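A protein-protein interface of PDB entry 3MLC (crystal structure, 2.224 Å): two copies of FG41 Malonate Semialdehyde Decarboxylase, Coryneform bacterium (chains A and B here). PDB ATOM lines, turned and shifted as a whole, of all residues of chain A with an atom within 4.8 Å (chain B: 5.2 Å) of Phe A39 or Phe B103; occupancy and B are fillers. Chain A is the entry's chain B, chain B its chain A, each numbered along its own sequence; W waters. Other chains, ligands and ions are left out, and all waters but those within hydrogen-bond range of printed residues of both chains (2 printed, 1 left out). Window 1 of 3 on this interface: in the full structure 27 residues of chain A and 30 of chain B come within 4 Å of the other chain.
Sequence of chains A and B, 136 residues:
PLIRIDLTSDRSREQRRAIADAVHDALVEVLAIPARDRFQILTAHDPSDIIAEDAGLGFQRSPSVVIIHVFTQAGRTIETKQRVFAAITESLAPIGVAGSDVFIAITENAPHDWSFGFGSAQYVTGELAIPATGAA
Water W1 lies within hydrogen-bond range of the guanidinium group (NH2) of Arg A36 and the backbone NH (N) of Asp B54.
Water W2 bridges OG of Ser A115 (2.8 Å) and O of Val B102 (3.3 Å).
O of Ile B51 sits at hydrogen-bond distance from N of Gln A40.
The side-chain carboxylate (OE1) of Glu B53 lies within salt-bridge range of the guanidinium group (NE) of Arg A36, 3.7 Å away.
The backbone NH of Glu B53 sits at hydrogen-bond distance from the backbone carbonyl oxygen of Arg A38, 3.1 Å away.
NH1 of Arg A36 is in salt-bridge range of OD2 of Asp B54, 3.2 Å away.
The backbone NH of Ala B55 sits at hydrogen-bond distance from the backbone carbonyl oxygen of Arg A36 (2.8 Å).
The guanidinium group of Arg B61 is in hydrogen-bond range of the backbone carbonyl oxygen of Phe A116, 2.6 Å away.
The backbone carbonyl oxygen (O) of Ile B104 lies within hydrogen-bond range of the backbone NH (N) of Ser A115, 2.8 Å away.
The backbone carbonyl oxygen (O) of Arg A38 lies close to the backbone carbonyl oxygen (O) of Ile B51 (3.2 Å).
Arg A38 touches Ala B52 (O to CA, 3.4 Å).
Ile B51 touches Phe A39 (O to CA, 3.2 Å).
O of Glu B53 touches CE2 of Phe A39, 3.0 Å away.
CE2 of Phe A39 touches NH2 of Arg B61, at 3.5 Å.
Phe B103 touches Phe A39.
Ile A41 touches Ile B67.
Phe B103 touches Trp A114.
C of Trp A114 touches O of Ile B104, at 3.7 Å.
Ala B105 touches Trp A114.
Phe A116 touches Phe B103 (CD1 to CE1, 3.6 Å).
NE of Arg B61 sits close to O of Ala B52 (3.0 Å).
O of Val B66 is in hydrogen-bond range of N of Phe B103 (3.1 Å).
The backbone carbonyl oxygen (O) of Phe B103 lies within hydrogen-bond range of the backbone NH (N) of Ile B68 (2.8 Å).
The backbone carbonyl oxygen (O) of Phe A39 sits at hydrogen-bond distance from the backbone NH (N) of Ile A3 (2.9 Å).
The backbone carbonyl oxygen of Ile A3 sits at hydrogen-bond distance from the backbone NH of Ile A41, 2.9 Å away.
NE of Arg A38 is in hydrogen-bond range of OE1 of Gln A40, 2.9 Å away.
No position is printed for both chains.
Of the 12 printed residues of chain A, 10 touch a printed residue of chain B.
Among the printed residues, 25 pairs touch across the chains.
Among the printed residues, Asp or Glu carboxylates within 4 Å of a Lys or Arg side-chain nitrogen of the other chain: Arg A36 with Glu B53 (3.7 Å) and Arg A36 with Asp B54 (3.2 Å).
Of the printed residues of chain B, Leu A2 touches Phe B103 (3.9 Å).
Phe A39 touches just these residues of chain B: Ile B51 (3.2 Å), Ala B52 (3.7 Å), Glu B53 (3.0 Å), Ala B55 (3.7 Å), Arg B61 (3.5 Å) and Phe B103 (3.5 Å).
Printed residues of chain A within 4 Å of Ala B52: Arg A38 and Phe A39.
Of the printed residues of chain A, Glu B53 touches Arg A36 (3.3 Å), Arg A38 (3.1 Å) and Phe A39 (3.0 Å).
Ile B68 touches none of the printed residues of chain A.
Printed residues of chain A within 4 Å of Val B102: Phe A116.
Phe B103 touches just these residues of chain A: Leu A2, Phe A39, Trp A114, Ser A115 and Phe A116.
Of the printed residues of chain A, Ile B104 touches Trp A114 and Ser A115.
The nearest printed residue of chain A that does not touch Phe B103 is Pro A1 (5.1 Å).
The nearest printed residue of chain A that does not touch Ile B104 is Phe A116 (5.0 Å).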
ATOM      1  N   PRO A   1       3.099  -5.092 -13.269  1.00  0.00           N
ATOM      2  CA  PRO A   1       4.465  -4.855 -12.815  1.00  0.00           C
ATOM      3  C   PRO A   1       4.550  -3.803 -11.706  1.00  0.00           C
ATOM      4  O   PRO A   1       3.608  -3.031 -11.506  1.00  0.00           O
ATOM      5  CB  PRO A   1       5.161  -4.347 -14.079  1.00  0.00           C
ATOM      6  CG  PRO A   1       4.082  -3.655 -14.840  1.00  0.00           C
ATOM      7  CD  PRO A   1       2.801  -4.389 -14.532  1.00  0.00           C
ATOM      8  N   LEU A   2       5.671  -3.797 -10.989  1.00  0.00           N
ATOM      9  CA  LEU A   2       5.956  -2.777  -9.981  1.00  0.00           C
ATOM     10  C   LEU A   2       7.084  -1.882 -10.484  1.00  0.00           C
ATOM     11  O   LEU A   2       8.138  -2.369 -10.903  1.00  0.00           O
ATOM     12  CB  LEU A   2       6.322  -3.412  -8.635  1.00  0.00           C
ATOM     13  CG  LEU A   2       6.712  -2.485  -7.475  1.00  0.00           C
ATOM     14  CD1 LEU A   2       5.503  -1.741  -6.908  1.00  0.00           C
ATOM     15  CD2 LEU A   2       7.422  -3.271  -6.382  1.00  0.00           C
ATOM     16  N   ILE A   3       6.966  -0.541 -10.465  1.00  0.00           N
ATOM     17  CA  ILE A   3       7.891   0.397 -11.061  1.00  0.00           C
ATOM     18  C   ILE A   3       8.449   1.286  -9.960  1.00  0.00           C
ATOM     19  O   ILE A   3       7.717   2.003  -9.301  1.00  0.00           O
ATOM     20  CB  ILE A   3       7.216   1.275 -12.185  1.00  0.00           C
ATOM     21  CG1 ILE A   3       6.250   0.453 -13.074  1.00  0.00           C
ATOM     22  CG2 ILE A   3       8.266   2.025 -13.000  1.00  0.00           C
ATOM     23  CD1 ILE A   3       6.879  -0.796 -13.798  1.00  0.00           C
ATOM     24  N   ARG A  36      -5.593  -0.338 -14.989  1.00  0.00           N
ATOM     25  CA  ARG A  36      -5.619  -0.231 -13.522  1.00  0.00           C
ATOM     26  C   ARG A  36      -4.513  -1.093 -12.858  1.00  0.00           C
ATOM     27  O   ARG A  36      -4.364  -1.110 -11.634  1.00  0.00           O
ATOM     28  CB  ARG A  36      -7.020  -0.573 -12.972  1.00  0.00           C
ATOM     29  CG  ARG A  36      -8.119   0.491 -13.263  1.00  0.00           C
ATOM     30  CD  ARG A  36      -9.044   0.704 -12.048  1.00  0.00           C
ATOM     31  NE  ARG A  36      -8.338   1.367 -10.939  1.00  0.00           N
ATOM     32  CZ  ARG A  36      -8.738   1.409  -9.658  1.00  0.00           C
ATOM     33  NH1 ARG A  36      -9.878   0.837  -9.262  1.00  0.00           N
ATOM     34  NH2 ARG A  36      -7.991   2.044  -8.760  1.00  0.00           N
ATOM     35  N   ASP A  37      -3.753  -1.797 -13.686  1.00  0.00           N
ATOM     36  CA  ASP A  37      -2.576  -2.531 -13.244  1.00  0.00           C
ATOM     37  C   ASP A  37      -1.404  -1.554 -13.090  1.00  0.00           C
ATOM     38  O   ASP A  37      -0.422  -1.603 -13.843  1.00  0.00           O
ATOM     39  CB  ASP A  37      -2.277  -3.674 -14.233  1.00  0.00           C
ATOM     40  CG  ASP A  37      -1.032  -4.463 -13.884  1.00  0.00           C
ATOM     41  OD1 ASP A  37      -0.521  -4.343 -12.745  1.00  0.00           O
ATOM     42  OD2 ASP A  37      -0.553  -5.213 -14.758  1.00  0.00           O
ATOM     43  N   ARG A  38      -1.539  -0.663 -12.098  1.00  0.00           N
ATOM     44  CA  ARG A  38      -0.617   0.456 -11.890  1.00  0.00           C
ATOM     45  C   ARG A  38      -0.030   0.437 -10.491  1.00  0.00           C
ATOM     46  O   ARG A  38      -0.739   0.752  -9.521  1.00  0.00           O
ATOM     47  CB  ARG A  38      -1.329   1.787 -12.119  1.00  0.00           C
ATOM     48  CG  ARG A  38      -0.357   2.964 -12.170  1.00  0.00           C
ATOM     49  CD  ARG A  38      -1.005   4.261 -12.525  1.00  0.00           C
ATOM     50  NE  ARG A  38      -0.010   5.320 -12.449  1.00  0.00           N
ATOM     51  CZ  ARG A  38      -0.221   6.618 -12.707  1.00  0.00           C
ATOM     52  NH1 ARG A  38      -1.419   7.080 -13.070  1.00  0.00           N
ATOM     53  NH2 ARG A  38       0.784   7.471 -12.589  1.00  0.00           N
ATOM     54  N   PHE A  39       1.250   0.052 -10.384  1.00  0.00           N
ATOM     55  CA  PHE A  39       1.948  -0.003  -9.088  1.00  0.00           C
ATOM     56  C   PHE A  39       3.308   0.682  -9.142  1.00  0.00           C
ATOM     57  O   PHE A  39       4.257   0.153  -9.720  1.00  0.00           O
ATOM     58  CB  PHE A  39       2.046  -1.449  -8.590  1.00  0.00           C
ATOM     59  CG  PHE A  39       0.748  -2.178  -8.710  1.00  0.00           C
ATOM     60  CD1 PHE A  39       0.490  -2.998  -9.817  1.00  0.00           C
ATOM     61  CD2 PHE A  39      -0.266  -1.964  -7.764  1.00  0.00           C
ATOM     62  CE1 PHE A  39      -0.747  -3.627  -9.952  1.00  0.00           C
ATOM     63  CE2 PHE A  39      -1.504  -2.577  -7.902  1.00  0.00           C
ATOM     64  CZ  PHE A  39      -1.753  -3.407  -8.987  1.00  0.00           C
ATOM     65  N   GLN A  40       3.371   1.874  -8.540  1.00  0.00           N
ATOM     66  CA  GLN A  40       4.522   2.790  -8.667  1.00  0.00           C
ATOM     67  C   GLN A  40       4.990   3.387  -7.351  1.00  0.00           C
ATOM     68  O   GLN A  40       4.178   3.753  -6.481  1.00  0.00           O
ATOM     69  CB  GLN A  40       4.236   3.906  -9.688  1.00  0.00           C
ATOM     70  CG  GLN A  40       3.882   3.373 -11.059  1.00  0.00           C
ATOM     71  CD  GLN A  40       3.444   4.427 -12.064  1.00  0.00           C
ATOM     72  OE1 GLN A  40       2.824   5.433 -11.715  1.00  0.00           O
ATOM     73  NE2 GLN A  40       3.747   4.175 -13.332  1.00  0.00           N
ATOM     74  N   ILE A  41       6.318   3.446  -7.199  1.00  0.00           N
ATOM     75  CA  ILE A  41       6.952   4.186  -6.092  1.00  0.00           C
ATOM     76  C   ILE A  41       7.806   5.295  -6.702  1.00  0.00           C
ATOM     77  O   ILE A  41       8.680   5.042  -7.521  1.00  0.00           O
ATOM     78  CB  ILE A  41       7.756   3.256  -5.135  1.00  0.00           C
ATOM     79  CG1 ILE A  41       6.841   2.132  -4.577  1.00  0.00           C
ATOM     80  CG2 ILE A  41       8.366   4.058  -3.986  1.00  0.00           C
ATOM     81  CD1 ILE A  41       7.546   0.827  -4.177  1.00  0.00           C
ATOM     82  N   TRP A 114       3.775 -12.643  -6.740  1.00  0.00           N
ATOM     83  CA  TRP A 114       2.970 -11.410  -6.729  1.00  0.00           C
ATOM     84  C   TRP A 114       1.708 -11.541  -5.867  1.00  0.00           C
ATOM     85  O   TRP A 114       0.952 -12.476  -6.046  1.00  0.00           O
ATOM     86  CB  TRP A 114       2.591 -11.050  -8.187  1.00  0.00           C
ATOM     87  CG  TRP A 114       3.775 -10.606  -9.054  1.00  0.00           C
ATOM     88  CD1 TRP A 114       4.482 -11.365  -9.963  1.00  0.00           C
ATOM     89  CD2 TRP A 114       4.387  -9.312  -9.057  1.00  0.00           C
ATOM     90  NE1 TRP A 114       5.486 -10.622 -10.521  1.00  0.00           N
ATOM     91  CE2 TRP A 114       5.443  -9.351  -9.994  1.00  0.00           C
ATOM     92  CE3 TRP A 114       4.129  -8.113  -8.375  1.00  0.00           C
ATOM     93  CZ2 TRP A 114       6.250  -8.239 -10.255  1.00  0.00           C
ATOM     94  CZ3 TRP A 114       4.944  -7.013  -8.626  1.00  0.00           C
ATOM     95  CH2 TRP A 114       5.993  -7.089  -9.559  1.00  0.00           C
ATOM     96  N   SER A 115       1.505 -10.638  -4.905  1.00  0.00           N
ATOM     97  CA  SER A 115       0.237 -10.546  -4.148  1.00  0.00           C
ATOM     98  C   SER A 115      -0.309  -9.115  -4.234  1.00  0.00           C
ATOM     99  O   SER A 115       0.313  -8.181  -3.721  1.00  0.00           O
ATOM    100  CB  SER A 115       0.446 -10.909  -2.682  1.00  0.00           C
ATOM    101  OG  SER A 115      -0.764 -10.773  -1.932  1.00  0.00           O
ATOM    102  N   PHE A 116      -1.471  -8.940  -4.870  1.00  0.00           N
ATOM    103  CA  PHE A 116      -1.973  -7.594  -5.148  1.00  0.00           C
ATOM    104  C   PHE A 116      -2.858  -7.068  -4.046  1.00  0.00           C
ATOM    105  O   PHE A 116      -3.390  -5.980  -4.161  1.00  0.00           O
ATOM    106  CB  PHE A 116      -2.714  -7.542  -6.493  1.00  0.00           C
ATOM    107  CG  PHE A 116      -1.834  -7.801  -7.684  1.00  0.00           C
ATOM    108  CD1 PHE A 116      -1.441  -6.762  -8.509  1.00  0.00           C
ATOM    109  CD2 PHE A 116      -1.397  -9.094  -7.980  1.00  0.00           C
ATOM    110  CE1 PHE A 116      -0.620  -7.004  -9.615  1.00  0.00           C
ATOM    111  CE2 PHE A 116      -0.583  -9.328  -9.073  1.00  0.00           C
ATOM    112  CZ  PHE A 116      -0.197  -8.281  -9.891  1.00  0.00           C
ATOM    113  N   ILE B  51       1.475   5.034  -5.928  1.00  0.00           N
ATOM    114  CA  ILE B  51       0.238   4.699  -6.625  1.00  0.00           C
ATOM    115  C   ILE B  51       0.083   3.179  -6.692  1.00  0.00           C
ATOM    116  O   ILE B  51       0.884   2.489  -7.322  1.00  0.00           O
ATOM    117  CB  ILE B  51       0.179   5.263  -8.089  1.00  0.00           C
ATOM    118  CG1 ILE B  51       0.252   6.787  -8.135  1.00  0.00           C
ATOM    119  CG2 ILE B  51      -1.128   4.819  -8.766  1.00  0.00           C
ATOM    120  CD1 ILE B  51       1.644   7.368  -8.169  1.00  0.00           C
ATOM    121  N   ALA B  52      -0.948   2.653  -6.041  1.00  0.00           N
ATOM    122  CA  ALA B  52      -1.251   1.232  -6.146  1.00  0.00           C
ATOM    123  C   ALA B  52      -2.752   1.075  -6.345  1.00  0.00           C
ATOM    124  O   ALA B  52      -3.543   1.171  -5.404  1.00  0.00           O
ATOM    125  CB  ALA B  52      -0.756   0.471  -4.925  1.00  0.00           C
ATOM    126  N   GLU B  53      -3.136   0.865  -7.596  1.00  0.00           N
ATOM    127  CA  GLU B  53      -4.534   0.693  -7.961  1.00  0.00           C
ATOM    128  C   GLU B  53      -4.931  -0.784  -7.804  1.00  0.00           C
ATOM    129  O   GLU B  53      -4.232  -1.546  -7.132  1.00  0.00           O
ATOM    130  CB  GLU B  53      -4.776   1.250  -9.367  1.00  0.00           C
ATOM    131  CG  GLU B  53      -4.430   2.749  -9.475  1.00  0.00           C
ATOM    132  CD  GLU B  53      -4.635   3.332 -10.865  1.00  0.00           C
ATOM    133  OE1 GLU B  53      -4.998   2.575 -11.786  1.00  0.00           O
ATOM    134  OE2 GLU B  53      -4.422   4.558 -11.039  1.00  0.00           O
ATOM    135  N   ASP B  54      -6.042  -1.204  -8.399  1.00  0.00           N
ATOM    136  CA  ASP B  54      -6.544  -2.554  -8.112  1.00  0.00           C
ATOM    137  C   ASP B  54      -6.151  -3.648  -9.116  1.00  0.00           C
ATOM    138  O   ASP B  54      -6.466  -4.815  -8.897  1.00  0.00           O
ATOM    139  CB  ASP B  54      -8.063  -2.535  -7.875  1.00  0.00           C
ATOM    140  CG  ASP B  54      -8.854  -2.275  -9.138  1.00  0.00           C
ATOM    141  OD1 ASP B  54     -10.081  -2.511  -9.131  1.00  0.00           O
ATOM    142  OD2 ASP B  54      -8.266  -1.843 -10.146  1.00  0.00           O
ATOM    143  N   ALA B  55      -5.457  -3.276 -10.193  1.00  0.00           N
ATOM    144  CA  ALA B  55      -5.212  -4.185 -11.338  1.00  0.00           C
ATOM    145  C   ALA B  55      -6.525  -4.681 -11.970  1.00  0.00           C
ATOM    146  O   ALA B  55      -6.580  -5.749 -12.584  1.00  0.00           O
ATOM    147  CB  ALA B  55      -4.283  -5.360 -10.946  1.00  0.00           C
ATOM    148  N   ARG B  61      -8.321   0.893  -2.581  1.00  0.00           N
ATOM    149  CA  ARG B  61      -7.410   0.993  -1.465  1.00  0.00           C
ATOM    150  C   ARG B  61      -7.604   2.356  -0.788  1.00  0.00           C
ATOM    151  O   ARG B  61      -8.092   3.324  -1.405  1.00  0.00           O
ATOM    152  CB  ARG B  61      -5.965   0.831  -1.966  1.00  0.00           C
ATOM    153  CG  ARG B  61      -5.765  -0.236  -3.054  1.00  0.00           C
ATOM    154  CD  ARG B  61      -4.283  -0.588  -3.176  1.00  0.00           C
ATOM    155  NE  ARG B  61      -3.991  -1.547  -4.247  1.00  0.00           N
ATOM    156  CZ  ARG B  61      -3.632  -2.820  -4.065  1.00  0.00           C
ATOM    157  NH1 ARG B  61      -3.521  -3.333  -2.844  1.00  0.00           N
ATOM    158  NH2 ARG B  61      -3.381  -3.598  -5.123  1.00  0.00           N
ATOM    159  N   VAL B  66       0.788   0.020   1.749  1.00  0.00           N
ATOM    160  CA  VAL B  66       2.060  -0.533   2.189  1.00  0.00           C
ATOM    161  C   VAL B  66       2.541  -1.490   1.103  1.00  0.00           C
ATOM    162  O   VAL B  66       1.885  -2.471   0.819  1.00  0.00           O
ATOM    163  CB  VAL B  66       1.928  -1.299   3.534  1.00  0.00           C
ATOM    164  CG1 VAL B  66       3.292  -1.831   4.026  1.00  0.00           C
ATOM    165  CG2 VAL B  66       1.287  -0.415   4.578  1.00  0.00           C
ATOM    166  N   ILE B  67       3.692  -1.186   0.505  1.00  0.00           N
ATOM    167  CA  ILE B  67       4.289  -2.043  -0.505  1.00  0.00           C
ATOM    168  C   ILE B  67       5.482  -2.746   0.104  1.00  0.00           C
ATOM    169  O   ILE B  67       6.364  -2.103   0.674  1.00  0.00           O
ATOM    170  CB  ILE B  67       4.699  -1.262  -1.810  1.00  0.00           C
ATOM    171  CG1 ILE B  67       3.479  -0.545  -2.411  1.00  0.00           C
ATOM    172  CG2 ILE B  67       5.340  -2.208  -2.831  1.00  0.00           C
ATOM    173  CD1 ILE B  67       3.718   0.035  -3.784  1.00  0.00           C
ATOM    174  N   ILE B  68       5.507  -4.070  -0.047  1.00  0.00           N
ATOM    175  CA  ILE B  68       6.486  -4.927   0.595  1.00  0.00           C
ATOM    176  C   ILE B  68       7.172  -5.745  -0.491  1.00  0.00           C
ATOM    177  O   ILE B  68       6.536  -6.502  -1.183  1.00  0.00           O
ATOM    178  CB  ILE B  68       5.808  -5.854   1.657  1.00  0.00           C
ATOM    179  CG1 ILE B  68       5.208  -5.032   2.798  1.00  0.00           C
ATOM    180  CG2 ILE B  68       6.781  -6.905   2.194  1.00  0.00           C
ATOM    181  CD1 ILE B  68       4.009  -5.688   3.492  1.00  0.00           C
ATOM    182  N   ASP B 101      -4.809  -2.758   1.332  1.00  0.00           N
ATOM    183  CA  ASP B 101      -3.691  -1.825   1.222  1.00  0.00           C
ATOM    184  C   ASP B 101      -2.318  -2.511   1.260  1.00  0.00           C
ATOM    185  O   ASP B 101      -1.306  -1.849   1.454  1.00  0.00           O
ATOM    186  CB  ASP B 101      -3.776  -0.766   2.331  1.00  0.00           C
ATOM    187  CG  ASP B 101      -5.059   0.043   2.288  1.00  0.00           C
ATOM    188  OD1 ASP B 101      -5.800  -0.042   1.289  1.00  0.00           O
ATOM    189  OD2 ASP B 101      -5.324   0.772   3.267  1.00  0.00           O
ATOM    190  N   VAL B 102      -2.288  -3.829   1.090  1.00  0.00           N
ATOM    191  CA  VAL B 102      -1.028  -4.569   1.118  1.00  0.00           C
ATOM    192  C   VAL B 102      -0.695  -5.070  -0.298  1.00  0.00           C
ATOM    193  O   VAL B 102      -1.511  -5.745  -0.935  1.00  0.00           O
ATOM    194  CB  VAL B 102      -1.086  -5.746   2.132  1.00  0.00           C
ATOM    195  CG1 VAL B 102       0.220  -6.558   2.132  1.00  0.00           C
ATOM    196  CG2 VAL B 102      -1.402  -5.237   3.545  1.00  0.00           C
ATOM    197  N   PHE B 103       0.489  -4.704  -0.789  1.00  0.00           N
ATOM    198  CA  PHE B 103       1.010  -5.196  -2.063  1.00  0.00           C
ATOM    199  C   PHE B 103       2.357  -5.866  -1.770  1.00  0.00           C
ATOM    200  O   PHE B 103       3.224  -5.278  -1.140  1.00  0.00           O
ATOM    201  CB  PHE B 103       1.169  -4.035  -3.057  1.00  0.00           C
ATOM    202  CG  PHE B 103       1.647  -4.452  -4.445  1.00  0.00           C
ATOM    203  CD1 PHE B 103       0.728  -4.680  -5.473  1.00  0.00           C
ATOM    204  CD2 PHE B 103       3.010  -4.588  -4.728  1.00  0.00           C
ATOM    205  CE1 PHE B 103       1.159  -5.043  -6.755  1.00  0.00           C
ATOM    206  CE2 PHE B 103       3.451  -4.961  -6.009  1.00  0.00           C
ATOM    207  CZ  PHE B 103       2.519  -5.179  -7.022  1.00  0.00           C
ATOM    208  N   ILE B 104       2.502  -7.119  -2.188  1.00  0.00           N
ATOM    209  CA  ILE B 104       3.747  -7.841  -1.961  1.00  0.00           C
ATOM    210  C   ILE B 104       4.278  -8.377  -3.277  1.00  0.00           C
ATOM    211  O   ILE B 104       3.514  -8.786  -4.158  1.00  0.00           O
ATOM    212  CB  ILE B 104       3.632  -9.014  -0.928  1.00  0.00           C
ATOM    213  CG1 ILE B 104       2.699  -8.672   0.246  1.00  0.00           C
ATOM    214  CG2 ILE B 104       5.034  -9.410  -0.379  1.00  0.00           C
ATOM    215  CD1 ILE B 104       2.208  -9.902   1.001  1.00  0.00           C
ATOM    216  N   ALA B 105       5.603  -8.357  -3.384  1.00  0.00           N
ATOM    217  CA  ALA B 105       6.332  -8.980  -4.471  1.00  0.00           C
ATOM    218  C   ALA B 105       7.613  -9.655  -3.968  1.00  0.00           C
ATOM    219  O   ALA B 105       8.215  -9.257  -2.958  1.00  0.00           O
ATOM    220  CB  ALA B 105       6.659  -7.945  -5.546  1.00  0.00           C
HETATM  221  O   HOH W   1      -7.983   0.387  -6.537  1.00  0.00           O
HETATM  222  O   HOH W   2      -1.450  -8.901   0.061  1.00  0.00           O
